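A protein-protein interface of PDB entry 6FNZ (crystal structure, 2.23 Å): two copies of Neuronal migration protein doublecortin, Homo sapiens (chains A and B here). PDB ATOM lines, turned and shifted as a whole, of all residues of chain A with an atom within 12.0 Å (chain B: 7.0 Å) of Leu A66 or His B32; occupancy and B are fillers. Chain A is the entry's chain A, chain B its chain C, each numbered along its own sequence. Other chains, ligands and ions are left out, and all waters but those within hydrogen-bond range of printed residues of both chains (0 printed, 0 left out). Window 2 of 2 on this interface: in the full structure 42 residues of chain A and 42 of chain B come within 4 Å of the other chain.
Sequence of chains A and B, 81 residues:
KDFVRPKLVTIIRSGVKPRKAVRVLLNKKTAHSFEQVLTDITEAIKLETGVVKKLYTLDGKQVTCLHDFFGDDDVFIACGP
Of the 11 printed residues of chain B, 6 touch a printed residue of chain A.
Hydrophobic or aromatic side chains of chain B within 4 Å of the printed part of chain A: Phe B34 and Val B37.
Along chain A the printed residues that touch a printed residue of chain B span positions 63 to 70.
Among the printed residues, 10 pairs touch across the chains.
No position is printed for both chains.
Of the 10 pairs that touch across the chains among the printed residues, none has its exchanged pair printed and touching as well.
CZ of Phe B34 touches O of Val A63 (3.1 Å).
Phe B34 touches Thr A64.
Cys A65 touches Phe B34 (C to CD1, 3.6 Å).
Leu A66 touches Ala B31 (CD1 to O, 3.7 Å).
CD1 of Leu A66 touches O of His B32, at 3.9 Å.
CD2 of Leu A66 touches O of Ser B33 (3.8 Å).
Phe B34 touches Leu A66 (N to CG, 3.8 Å).
Leu A66 touches Val B37.
CG1 of Val B37 touches CZ of Phe A69 (3.6 Å).
CE1 of Phe A70 touches N of Lys B28, at 3.6 Å.
Printed residues of chain B within 4 Å of Thr A64: Phe B34.
Printed residues of chain B within 4 Å of Leu A66: Ala B31, His B32, Ser B33, Phe B34 and Val B37.
Asp A68 touches none of the printed residues of chain B.
Of the printed residues of chain B, Phe A70 touches Lys B28 (3.6 Å).
Asn B27 touches none of the printed residues of chain A.
No residue of chain A comes within 4 Å of Thr B30.
Of the printed residues of chain A, Ala B31 touches Leu A66.
Of chain A, only Leu A66 (3.9 Å) comes within 4 Å of His B32.
Ser B33 touches just one residue of chain A: Leu A66.
Phe B34 touches just these residues of chain A: Val A63, Thr A64, Cys A65 and Leu A66.
The side-chain sulfur (SG) of Cys A65 lies close to the backbone NH (N) of His A67.
OG of Ser B33 lies within hydrogen-bond range of N of Gln B36 (3.1 Å).
A ring nitrogen (ND1) of His B32 lies within hydrogen-bond range of the backbone carbonyl oxygen (O) of Thr B30, at 2.9 Å.
The side-chain sulfur (SG) of Cys A65 sits at hydrogen-bond distance from the side-chain carboxylate (OD2) of Asp A68.
N of Thr A64 is in hydrogen-bond range of OD2 of Asp A68.
The backbone NH (N) of Val A63 sits at hydrogen-bond distance from the backbone carbonyl oxygen (O) of Leu A55 (2.8 Å).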
ATOM      1  N   LYS A  53      -3.889   1.934  12.138  1.00  0.00           N
ATOM      2  CA  LYS A  53      -4.136   1.979  13.576  1.00  0.00           C
ATOM      3  C   LYS A  53      -2.860   2.092  14.411  1.00  0.00           C
ATOM      4  O   LYS A  53      -2.884   2.707  15.483  1.00  0.00           O
ATOM      5  CB  LYS A  53      -4.917   0.733  14.020  1.00  0.00           C
ATOM      6  CG  LYS A  53      -6.293   0.560  13.363  1.00  0.00           C
ATOM      7  CD  LYS A  53      -7.370   1.396  14.051  1.00  0.00           C
ATOM      8  CE  LYS A  53      -8.762   1.032  13.551  1.00  0.00           C
ATOM      9  NZ  LYS A  53      -9.829   1.310  14.573  1.00  0.00           N
ATOM     10  N   LYS A  54      -1.746   1.521  13.960  1.00  0.00           N
ATOM     11  CA  LYS A  54      -0.508   1.577  14.716  1.00  0.00           C
ATOM     12  C   LYS A  54       0.648   1.912  13.777  1.00  0.00           C
ATOM     13  O   LYS A  54       0.572   1.710  12.560  1.00  0.00           O
ATOM     14  CB  LYS A  54      -0.232   0.249  15.448  1.00  0.00           C
ATOM     15  CG  LYS A  54      -1.311  -0.200  16.446  1.00  0.00           C
ATOM     16  CD  LYS A  54      -0.977  -1.591  17.003  1.00  0.00           C
ATOM     17  CE  LYS A  54      -2.069  -2.143  17.931  1.00  0.00           C
ATOM     18  NZ  LYS A  54      -1.902  -1.727  19.365  1.00  0.00           N
ATOM     19  N   LEU A  55       1.723   2.439  14.365  1.00  0.00           N
ATOM     20  CA  LEU A  55       2.988   2.683  13.687  1.00  0.00           C
ATOM     21  C   LEU A  55       4.120   2.100  14.517  1.00  0.00           C
ATOM     22  O   LEU A  55       4.086   2.143  15.748  1.00  0.00           O
ATOM     23  CB  LEU A  55       3.273   4.166  13.497  1.00  0.00           C
ATOM     24  CG  LEU A  55       2.782   5.002  12.336  1.00  0.00           C
ATOM     25  CD1 LEU A  55       3.454   6.357  12.496  1.00  0.00           C
ATOM     26  CD2 LEU A  55       3.174   4.379  11.017  1.00  0.00           C
ATOM     27  N   THR A  57       8.627   1.717  14.635  1.00  0.00           N
ATOM     28  CA  THR A  57       9.956   1.934  14.090  1.00  0.00           C
ATOM     29  C   THR A  57      10.445   0.655  13.424  1.00  0.00           C
ATOM     30  O   THR A  57       9.863  -0.424  13.583  1.00  0.00           O
ATOM     31  CB  THR A  57      10.951   2.332  15.179  1.00  0.00           C
ATOM     32  OG1 THR A  57      11.121   1.228  16.069  1.00  0.00           O
ATOM     33  CG2 THR A  57      10.467   3.539  15.963  1.00  0.00           C
ATOM     34  N   GLN A  62       6.742   0.767  19.243  1.00  0.00           N
ATOM     35  CA  GLN A  62       5.527   1.432  18.800  1.00  0.00           C
ATOM     36  C   GLN A  62       5.692   2.941  18.899  1.00  0.00           C
ATOM     37  O   GLN A  62       6.202   3.461  19.892  1.00  0.00           O
ATOM     38  CB  GLN A  62       4.322   0.980  19.626  1.00  0.00           C
ATOM     39  CG  GLN A  62       3.000   1.471  19.048  1.00  0.00           C
ATOM     40  CD  GLN A  62       1.800   0.776  19.651  1.00  0.00           C
ATOM     41  OE1 GLN A  62       1.932  -0.198  20.394  1.00  0.00           O
ATOM     42  NE2 GLN A  62       0.614   1.270  19.325  1.00  0.00           N
ATOM     43  N   VAL A  63       5.263   3.641  17.862  1.00  0.00           N
ATOM     44  CA  VAL A  63       5.210   5.093  17.854  1.00  0.00           C
ATOM     45  C   VAL A  63       3.788   5.496  18.221  1.00  0.00           C
ATOM     46  O   VAL A  63       2.844   5.191  17.485  1.00  0.00           O
ATOM     47  CB  VAL A  63       5.629   5.646  16.485  1.00  0.00           C
ATOM     48  CG1 VAL A  63       5.338   7.136  16.367  1.00  0.00           C
ATOM     49  CG2 VAL A  63       7.081   5.371  16.281  1.00  0.00           C
ATOM     50  N   THR A  64       3.634   6.175  19.359  1.00  0.00           N
ATOM     51  CA  THR A  64       2.323   6.440  19.937  1.00  0.00           C
ATOM     52  C   THR A  64       2.000   7.913  20.137  1.00  0.00           C
ATOM     53  O   THR A  64       0.915   8.222  20.645  1.00  0.00           O
ATOM     54  CB  THR A  64       2.186   5.725  21.292  1.00  0.00           C
ATOM     55  OG1 THR A  64       3.396   5.886  22.052  1.00  0.00           O
ATOM     56  CG2 THR A  64       1.910   4.256  21.081  1.00  0.00           C
ATOM     57  N   CYS A  65       2.890   8.832  19.772  1.00  0.00           N
ATOM     58  CA  CYS A  65       2.592  10.237  20.001  1.00  0.00           C
ATOM     59  C   CYS A  65       3.410  11.075  19.040  1.00  0.00           C
ATOM     60  O   CYS A  65       4.410  10.616  18.483  1.00  0.00           O
ATOM     61  CB  CYS A  65       2.896  10.650  21.440  1.00  0.00           C
ATOM     62  SG  CYS A  65       4.661  10.660  21.742  1.00  0.00           S
ATOM     63  N   LEU A  66       2.980  12.332  18.885  1.00  0.00           N
ATOM     64  CA  LEU A  66       3.660  13.258  17.981  1.00  0.00           C
ATOM     65  C   LEU A  66       5.140  13.401  18.303  1.00  0.00           C
ATOM     66  O   LEU A  66       5.949  13.649  17.398  1.00  0.00           O
ATOM     67  CB  LEU A  66       2.998  14.631  18.033  1.00  0.00           C
ATOM     68  CG  LEU A  66       1.627  14.782  17.388  1.00  0.00           C
ATOM     69  CD1 LEU A  66       1.082  16.172  17.654  1.00  0.00           C
ATOM     70  CD2 LEU A  66       1.715  14.538  15.896  1.00  0.00           C
ATOM     71  N   HIS A  67       5.519  13.258  19.572  1.00  0.00           N
ATOM     72  CA  HIS A  67       6.926  13.419  19.918  1.00  0.00           C
ATOM     73  C   HIS A  67       7.778  12.298  19.328  1.00  0.00           C
ATOM     74  O   HIS A  67       8.822  12.559  18.719  1.00  0.00           O
ATOM     75  CB  HIS A  67       7.105  13.489  21.431  1.00  0.00           C
ATOM     76  CG  HIS A  67       8.526  13.706  21.840  1.00  0.00           C
ATOM     77  ND1 HIS A  67       9.248  14.815  21.454  1.00  0.00           N
ATOM     78  CD2 HIS A  67       9.371  12.940  22.571  1.00  0.00           C
ATOM     79  CE1 HIS A  67      10.472  14.730  21.945  1.00  0.00           C
ATOM     80  NE2 HIS A  67      10.571  13.604  22.628  1.00  0.00           N
ATOM     81  N   ASP A  68       7.361  11.039  19.510  1.00  0.00           N
ATOM     82  CA  ASP A  68       8.066   9.932  18.864  1.00  0.00           C
ATOM     83  C   ASP A  68       8.101  10.101  17.350  1.00  0.00           C
ATOM     84  O   ASP A  68       9.056   9.673  16.691  1.00  0.00           O
ATOM     85  CB  ASP A  68       7.400   8.590  19.188  1.00  0.00           C
ATOM     86  CG  ASP A  68       7.187   8.364  20.659  1.00  0.00           C
ATOM     87  OD1 ASP A  68       8.027   8.831  21.461  1.00  0.00           O
ATOM     88  OD2 ASP A  68       6.176   7.701  20.999  1.00  0.00           O
ATOM     89  N   PHE A  69       7.054  10.690  16.777  1.00  0.00           N
ATOM     90  CA  PHE A  69       6.939  10.703  15.328  1.00  0.00           C
ATOM     91  C   PHE A  69       7.923  11.666  14.700  1.00  0.00           C
ATOM     92  O   PHE A  69       8.367  11.436  13.574  1.00  0.00           O
ATOM     93  CB  PHE A  69       5.513  11.062  14.910  1.00  0.00           C
ATOM     94  CG  PHE A  69       5.274  10.957  13.437  1.00  0.00           C
ATOM     95  CD1 PHE A  69       4.924   9.749  12.867  1.00  0.00           C
ATOM     96  CD2 PHE A  69       5.401  12.064  12.620  1.00  0.00           C
ATOM     97  CE1 PHE A  69       4.709   9.645  11.506  1.00  0.00           C
ATOM     98  CE2 PHE A  69       5.182  11.962  11.241  1.00  0.00           C
ATOM     99  CZ  PHE A  69       4.841  10.752  10.691  1.00  0.00           C
ATOM    100  N   PHE A  70       8.274  12.746  15.394  1.00  0.00           N
ATOM    101  CA  PHE A  70       9.128  13.769  14.813  1.00  0.00           C
ATOM    102  C   PHE A  70      10.556  13.678  15.315  1.00  0.00           C
ATOM    103  O   PHE A  70      11.311  14.646  15.200  1.00  0.00           O
ATOM    104  CB  PHE A  70       8.532  15.154  15.066  1.00  0.00           C
ATOM    105  CG  PHE A  70       7.327  15.427  14.221  1.00  0.00           C
ATOM    106  CD1 PHE A  70       7.470  15.825  12.896  1.00  0.00           C
ATOM    107  CD2 PHE A  70       6.053  15.231  14.723  1.00  0.00           C
ATOM    108  CE1 PHE A  70       6.356  16.054  12.093  1.00  0.00           C
ATOM    109  CE2 PHE A  70       4.938  15.454  13.932  1.00  0.00           C
ATOM    110  CZ  PHE A  70       5.091  15.867  12.612  1.00  0.00           C
ATOM    111  N   GLY A  71      10.941  12.523  15.850  1.00  0.00           N
ATOM    112  CA  GLY A  71      12.302  12.279  16.285  1.00  0.00           C
ATOM    113  C   GLY A  71      13.223  11.955  15.129  1.00  0.00           C
ATOM    114  O   GLY A  71      13.012  12.388  13.992  1.00  0.00           O
ATOM    115  N   ASP A  72      14.247  11.153  15.414  1.00  0.00           N
ATOM    116  CA  ASP A  72      15.335  10.976  14.460  1.00  0.00           C
ATOM    117  C   ASP A  72      14.941  10.089  13.281  1.00  0.00           C
ATOM    118  O   ASP A  72      15.301  10.386  12.133  1.00  0.00           O
ATOM    119  CB  ASP A  72      16.554  10.416  15.190  1.00  0.00           C
ATOM    120  CG  ASP A  72      17.088  11.379  16.246  1.00  0.00           C
ATOM    121  OD1 ASP A  72      17.265  12.576  15.918  1.00  0.00           O
ATOM    122  OD2 ASP A  72      17.306  10.944  17.403  1.00  0.00           O
ATOM    123  N   ASP A  73      14.209   8.999  13.535  1.00  0.00           N
ATOM    124  CA  ASP A  73      13.825   8.097  12.458  1.00  0.00           C
ATOM    125  C   ASP A  73      12.861   8.796  11.506  1.00  0.00           C
ATOM    126  O   ASP A  73      11.958   9.518  11.940  1.00  0.00           O
ATOM    127  CB  ASP A  73      13.169   6.836  13.024  1.00  0.00           C
ATOM    128  CG  ASP A  73      14.130   5.988  13.826  1.00  0.00           C
ATOM    129  OD1 ASP A  73      15.273   6.461  14.054  1.00  0.00           O
ATOM    130  OD2 ASP A  73      13.742   4.852  14.223  1.00  0.00           O
ATOM    131  N   ASP A  74      13.052   8.591  10.197  1.00  0.00           N
ATOM    132  CA  ASP A  74      12.067   9.059   9.221  1.00  0.00           C
ATOM    133  C   ASP A  74      11.472   7.928   8.388  1.00  0.00           C
ATOM    134  O   ASP A  74      10.833   8.204   7.365  1.00  0.00           O
ATOM    135  CB  ASP A  74      12.660  10.147   8.304  1.00  0.00           C
ATOM    136  CG  ASP A  74      13.799   9.642   7.419  1.00  0.00           C
ATOM    137  OD1 ASP A  74      13.692   8.585   6.760  1.00  0.00           O
ATOM    138  OD2 ASP A  74      14.824  10.336   7.345  1.00  0.00           O
ATOM    139  N   PHE A  76       9.038   4.386   8.864  1.00  0.00           N
ATOM    140  CA  PHE A  76       8.167   3.730   9.833  1.00  0.00           C
ATOM    141  C   PHE A  76       7.377   2.617   9.164  1.00  0.00           C
ATOM    142  O   PHE A  76       7.153   2.627   7.950  1.00  0.00           O
ATOM    143  CB  PHE A  76       7.186   4.719  10.478  1.00  0.00           C
ATOM    144  CG  PHE A  76       7.847   5.793  11.289  1.00  0.00           C
ATOM    145  CD1 PHE A  76       8.526   5.477  12.461  1.00  0.00           C
ATOM    146  CD2 PHE A  76       7.778   7.120  10.890  1.00  0.00           C
ATOM    147  CE1 PHE A  76       9.157   6.486  13.229  1.00  0.00           C
ATOM    148  CE2 PHE A  76       8.384   8.132  11.638  1.00  0.00           C
ATOM    149  CZ  PHE A  76       9.081   7.815  12.814  1.00  0.00           C
ATOM    150  N   ASN B  27       4.290  18.458   8.746  1.00  0.00           N
ATOM    151  CA  ASN B  27       4.876  19.592   9.450  1.00  0.00           C
ATOM    152  C   ASN B  27       4.541  19.503  10.934  1.00  0.00           C
ATOM    153  O   ASN B  27       3.367  19.366  11.301  1.00  0.00           O
ATOM    154  CB  ASN B  27       4.372  20.913   8.865  1.00  0.00           C
ATOM    155  CG  ASN B  27       5.309  22.066   9.150  1.00  0.00           C
ATOM    156  OD1 ASN B  27       5.136  22.788  10.127  1.00  0.00           O
ATOM    157  ND2 ASN B  27       6.314  22.242   8.300  1.00  0.00           N
ATOM    158  N   LYS B  28       5.576  19.585  11.780  1.00  0.00           N
ATOM    159  CA  LYS B  28       5.397  19.454  13.229  1.00  0.00           C
ATOM    160  C   LYS B  28       4.408  20.476  13.772  1.00  0.00           C
ATOM    161  O   LYS B  28       3.743  20.223  14.783  1.00  0.00           O
ATOM    162  CB  LYS B  28       6.751  19.596  13.931  1.00  0.00           C
ATOM    163  CG  LYS B  28       6.769  19.215  15.406  1.00  0.00           C
ATOM    164  CD  LYS B  28       8.210  19.092  15.911  1.00  0.00           C
ATOM    165  CE  LYS B  28       8.273  18.879  17.421  1.00  0.00           C
ATOM    166  NZ  LYS B  28       7.717  20.045  18.168  1.00  0.00           N
ATOM    167  N   LYS B  29       4.285  21.621  13.104  1.00  0.00           N
ATOM    168  CA  LYS B  29       3.351  22.659  13.520  1.00  0.00           C
ATOM    169  C   LYS B  29       1.934  22.363  13.030  1.00  0.00           C
ATOM    170  O   LYS B  29       0.970  22.464  13.797  1.00  0.00           O
ATOM    171  CB  LYS B  29       3.845  24.017  13.009  1.00  0.00           C
ATOM    172  CG  LYS B  29       5.354  24.231  13.202  1.00  0.00           C
ATOM    173  CD  LYS B  29       5.964  25.134  12.126  1.00  0.00           C
ATOM    174  CE  LYS B  29       7.421  24.758  11.835  1.00  0.00           C
ATOM    175  NZ  LYS B  29       8.002  25.511  10.685  1.00  0.00           N
ATOM    176  N   THR B  30       1.789  21.976  11.760  1.00  0.00           N
ATOM    177  CA  THR B  30       0.458  21.786  11.190  1.00  0.00           C
ATOM    178  C   THR B  30      -0.212  20.513  11.701  1.00  0.00           C
ATOM    179  O   THR B  30      -1.445  20.442  11.748  1.00  0.00           O
ATOM    180  CB  THR B  30       0.541  21.771   9.661  1.00  0.00           C
ATOM    181  OG1 THR B  30       1.134  20.541   9.210  1.00  0.00           O
ATOM    182  CG2 THR B  30       1.385  22.941   9.171  1.00  0.00           C
ATOM    183  N   ALA B  31       0.567  19.503  12.084  1.00  0.00           N
ATOM    184  CA  ALA B  31       0.020  18.239  12.573  1.00  0.00           C
ATOM    185  C   ALA B  31      -0.538  18.447  13.972  1.00  0.00           C
ATOM    186  O   ALA B  31       0.212  18.542  14.944  1.00  0.00           O
ATOM    187  CB  ALA B  31       1.093  17.159  12.572  1.00  0.00           C
ATOM    188  N   HIS B  32      -1.864  18.500  14.086  1.00  0.00           N
ATOM    189  CA  HIS B  32      -2.458  18.904  15.354  1.00  0.00           C
ATOM    190  C   HIS B  32      -2.510  17.759  16.356  1.00  0.00           C
ATOM    191  O   HIS B  32      -2.338  17.981  17.557  1.00  0.00           O
ATOM    192  CB  HIS B  32      -3.849  19.485  15.115  1.00  0.00           C
ATOM    193  CG  HIS B  32      -3.819  20.830  14.464  1.00  0.00           C
ATOM    194  ND1 HIS B  32      -2.640  21.476  14.163  1.00  0.00           N
ATOM    195  CD2 HIS B  32      -4.815  21.653  14.062  1.00  0.00           C
ATOM    196  CE1 HIS B  32      -2.912  22.639  13.600  1.00  0.00           C
ATOM    197  NE2 HIS B  32      -4.224  22.772  13.528  1.00  0.00           N
ATOM    198  N   SER B  33      -2.743  16.535  15.900  1.00  0.00           N
ATOM    199  CA  SER B  33      -2.787  15.404  16.807  1.00  0.00           C
ATOM    200  C   SER B  33      -2.123  14.211  16.148  1.00  0.00           C
ATOM    201  O   SER B  33      -1.919  14.171  14.932  1.00  0.00           O
ATOM    202  CB  SER B  33      -4.219  15.045  17.202  1.00  0.00           C
ATOM    203  OG  SER B  33      -4.976  14.698  16.058  1.00  0.00           O
ATOM    204  N   PHE B  34      -1.800  13.223  16.979  1.00  0.00           N
ATOM    205  CA  PHE B  34      -1.285  11.966  16.458  1.00  0.00           C
ATOM    206  C   PHE B  34      -2.310  11.272  15.567  1.00  0.00           C
ATOM    207  O   PHE B  34      -1.950  10.663  14.551  1.00  0.00           O
ATOM    208  CB  PHE B  34      -0.880  11.061  17.611  1.00  0.00           C
ATOM    209  CG  PHE B  34      -0.124   9.856  17.180  1.00  0.00           C
ATOM    210  CD1 PHE B  34       1.081   9.989  16.509  1.00  0.00           C
ATOM    211  CD2 PHE B  34      -0.606   8.587  17.450  1.00  0.00           C
ATOM    212  CE1 PHE B  34       1.798   8.877  16.110  1.00  0.00           C
ATOM    213  CE2 PHE B  34       0.106   7.467  17.054  1.00  0.00           C
ATOM    214  CZ  PHE B  34       1.310   7.613  16.384  1.00  0.00           C
ATOM    215  N   GLU B  35      -3.591  11.354  15.933  1.00  0.00           N
ATOM    216  CA  GLU B  35      -4.646  10.767  15.112  1.00  0.00           C
ATOM    217  C   GLU B  35      -4.701  11.425  13.744  1.00  0.00           C
ATOM    218  O   GLU B  35      -4.922  10.751  12.730  1.00  0.00           O
ATOM    219  CB  GLU B  35      -6.003  10.900  15.806  1.00  0.00           C
ATOM    220  CG  GLU B  35      -5.936  10.987  17.319  1.00  0.00           C
ATOM    221  CD  GLU B  35      -5.292   9.768  17.946  1.00  0.00           C
ATOM    222  OE1 GLU B  35      -5.406   8.664  17.361  1.00  0.00           O
ATOM    223  OE2 GLU B  35      -4.662   9.923  19.018  1.00  0.00           O
ATOM    224  N   GLN B  36      -4.516  12.746  13.704  1.00  0.00           N
ATOM    225  CA  GLN B  36      -4.417  13.437  12.426  1.00  0.00           C
ATOM    226  C   GLN B  36      -3.313  12.837  11.562  1.00  0.00           C
ATOM    227  O   GLN B  36      -3.501  12.627  10.359  1.00  0.00           O
ATOM    228  CB  GLN B  36      -4.166  14.926  12.654  1.00  0.00           C
ATOM    229  CG  GLN B  36      -4.338  15.763  11.409  1.00  0.00           C
ATOM    230  CD  GLN B  36      -5.763  15.729  10.903  1.00  0.00           C
ATOM    231  OE1 GLN B  36      -6.132  14.871  10.102  1.00  0.00           O
ATOM    232  NE2 GLN B  36      -6.580  16.662  11.381  1.00  0.00           N
ATOM    233  N   VAL B  37      -2.154  12.550  12.161  1.00  0.00           N
ATOM    234  CA  VAL B  37      -1.031  12.011  11.397  1.00  0.00           C
ATOM    235  C   VAL B  37      -1.381  10.638  10.834  1.00  0.00           C
ATOM    236  O   VAL B  37      -1.102  10.342   9.667  1.00  0.00           O
ATOM    237  CB  VAL B  37       0.242  11.960  12.264  1.00  0.00           C
ATOM    238  CG1 VAL B  37       1.321  11.149  11.571  1.00  0.00           C
ATOM    239  CG2 VAL B  37       0.755  13.371  12.553  1.00  0.00           C
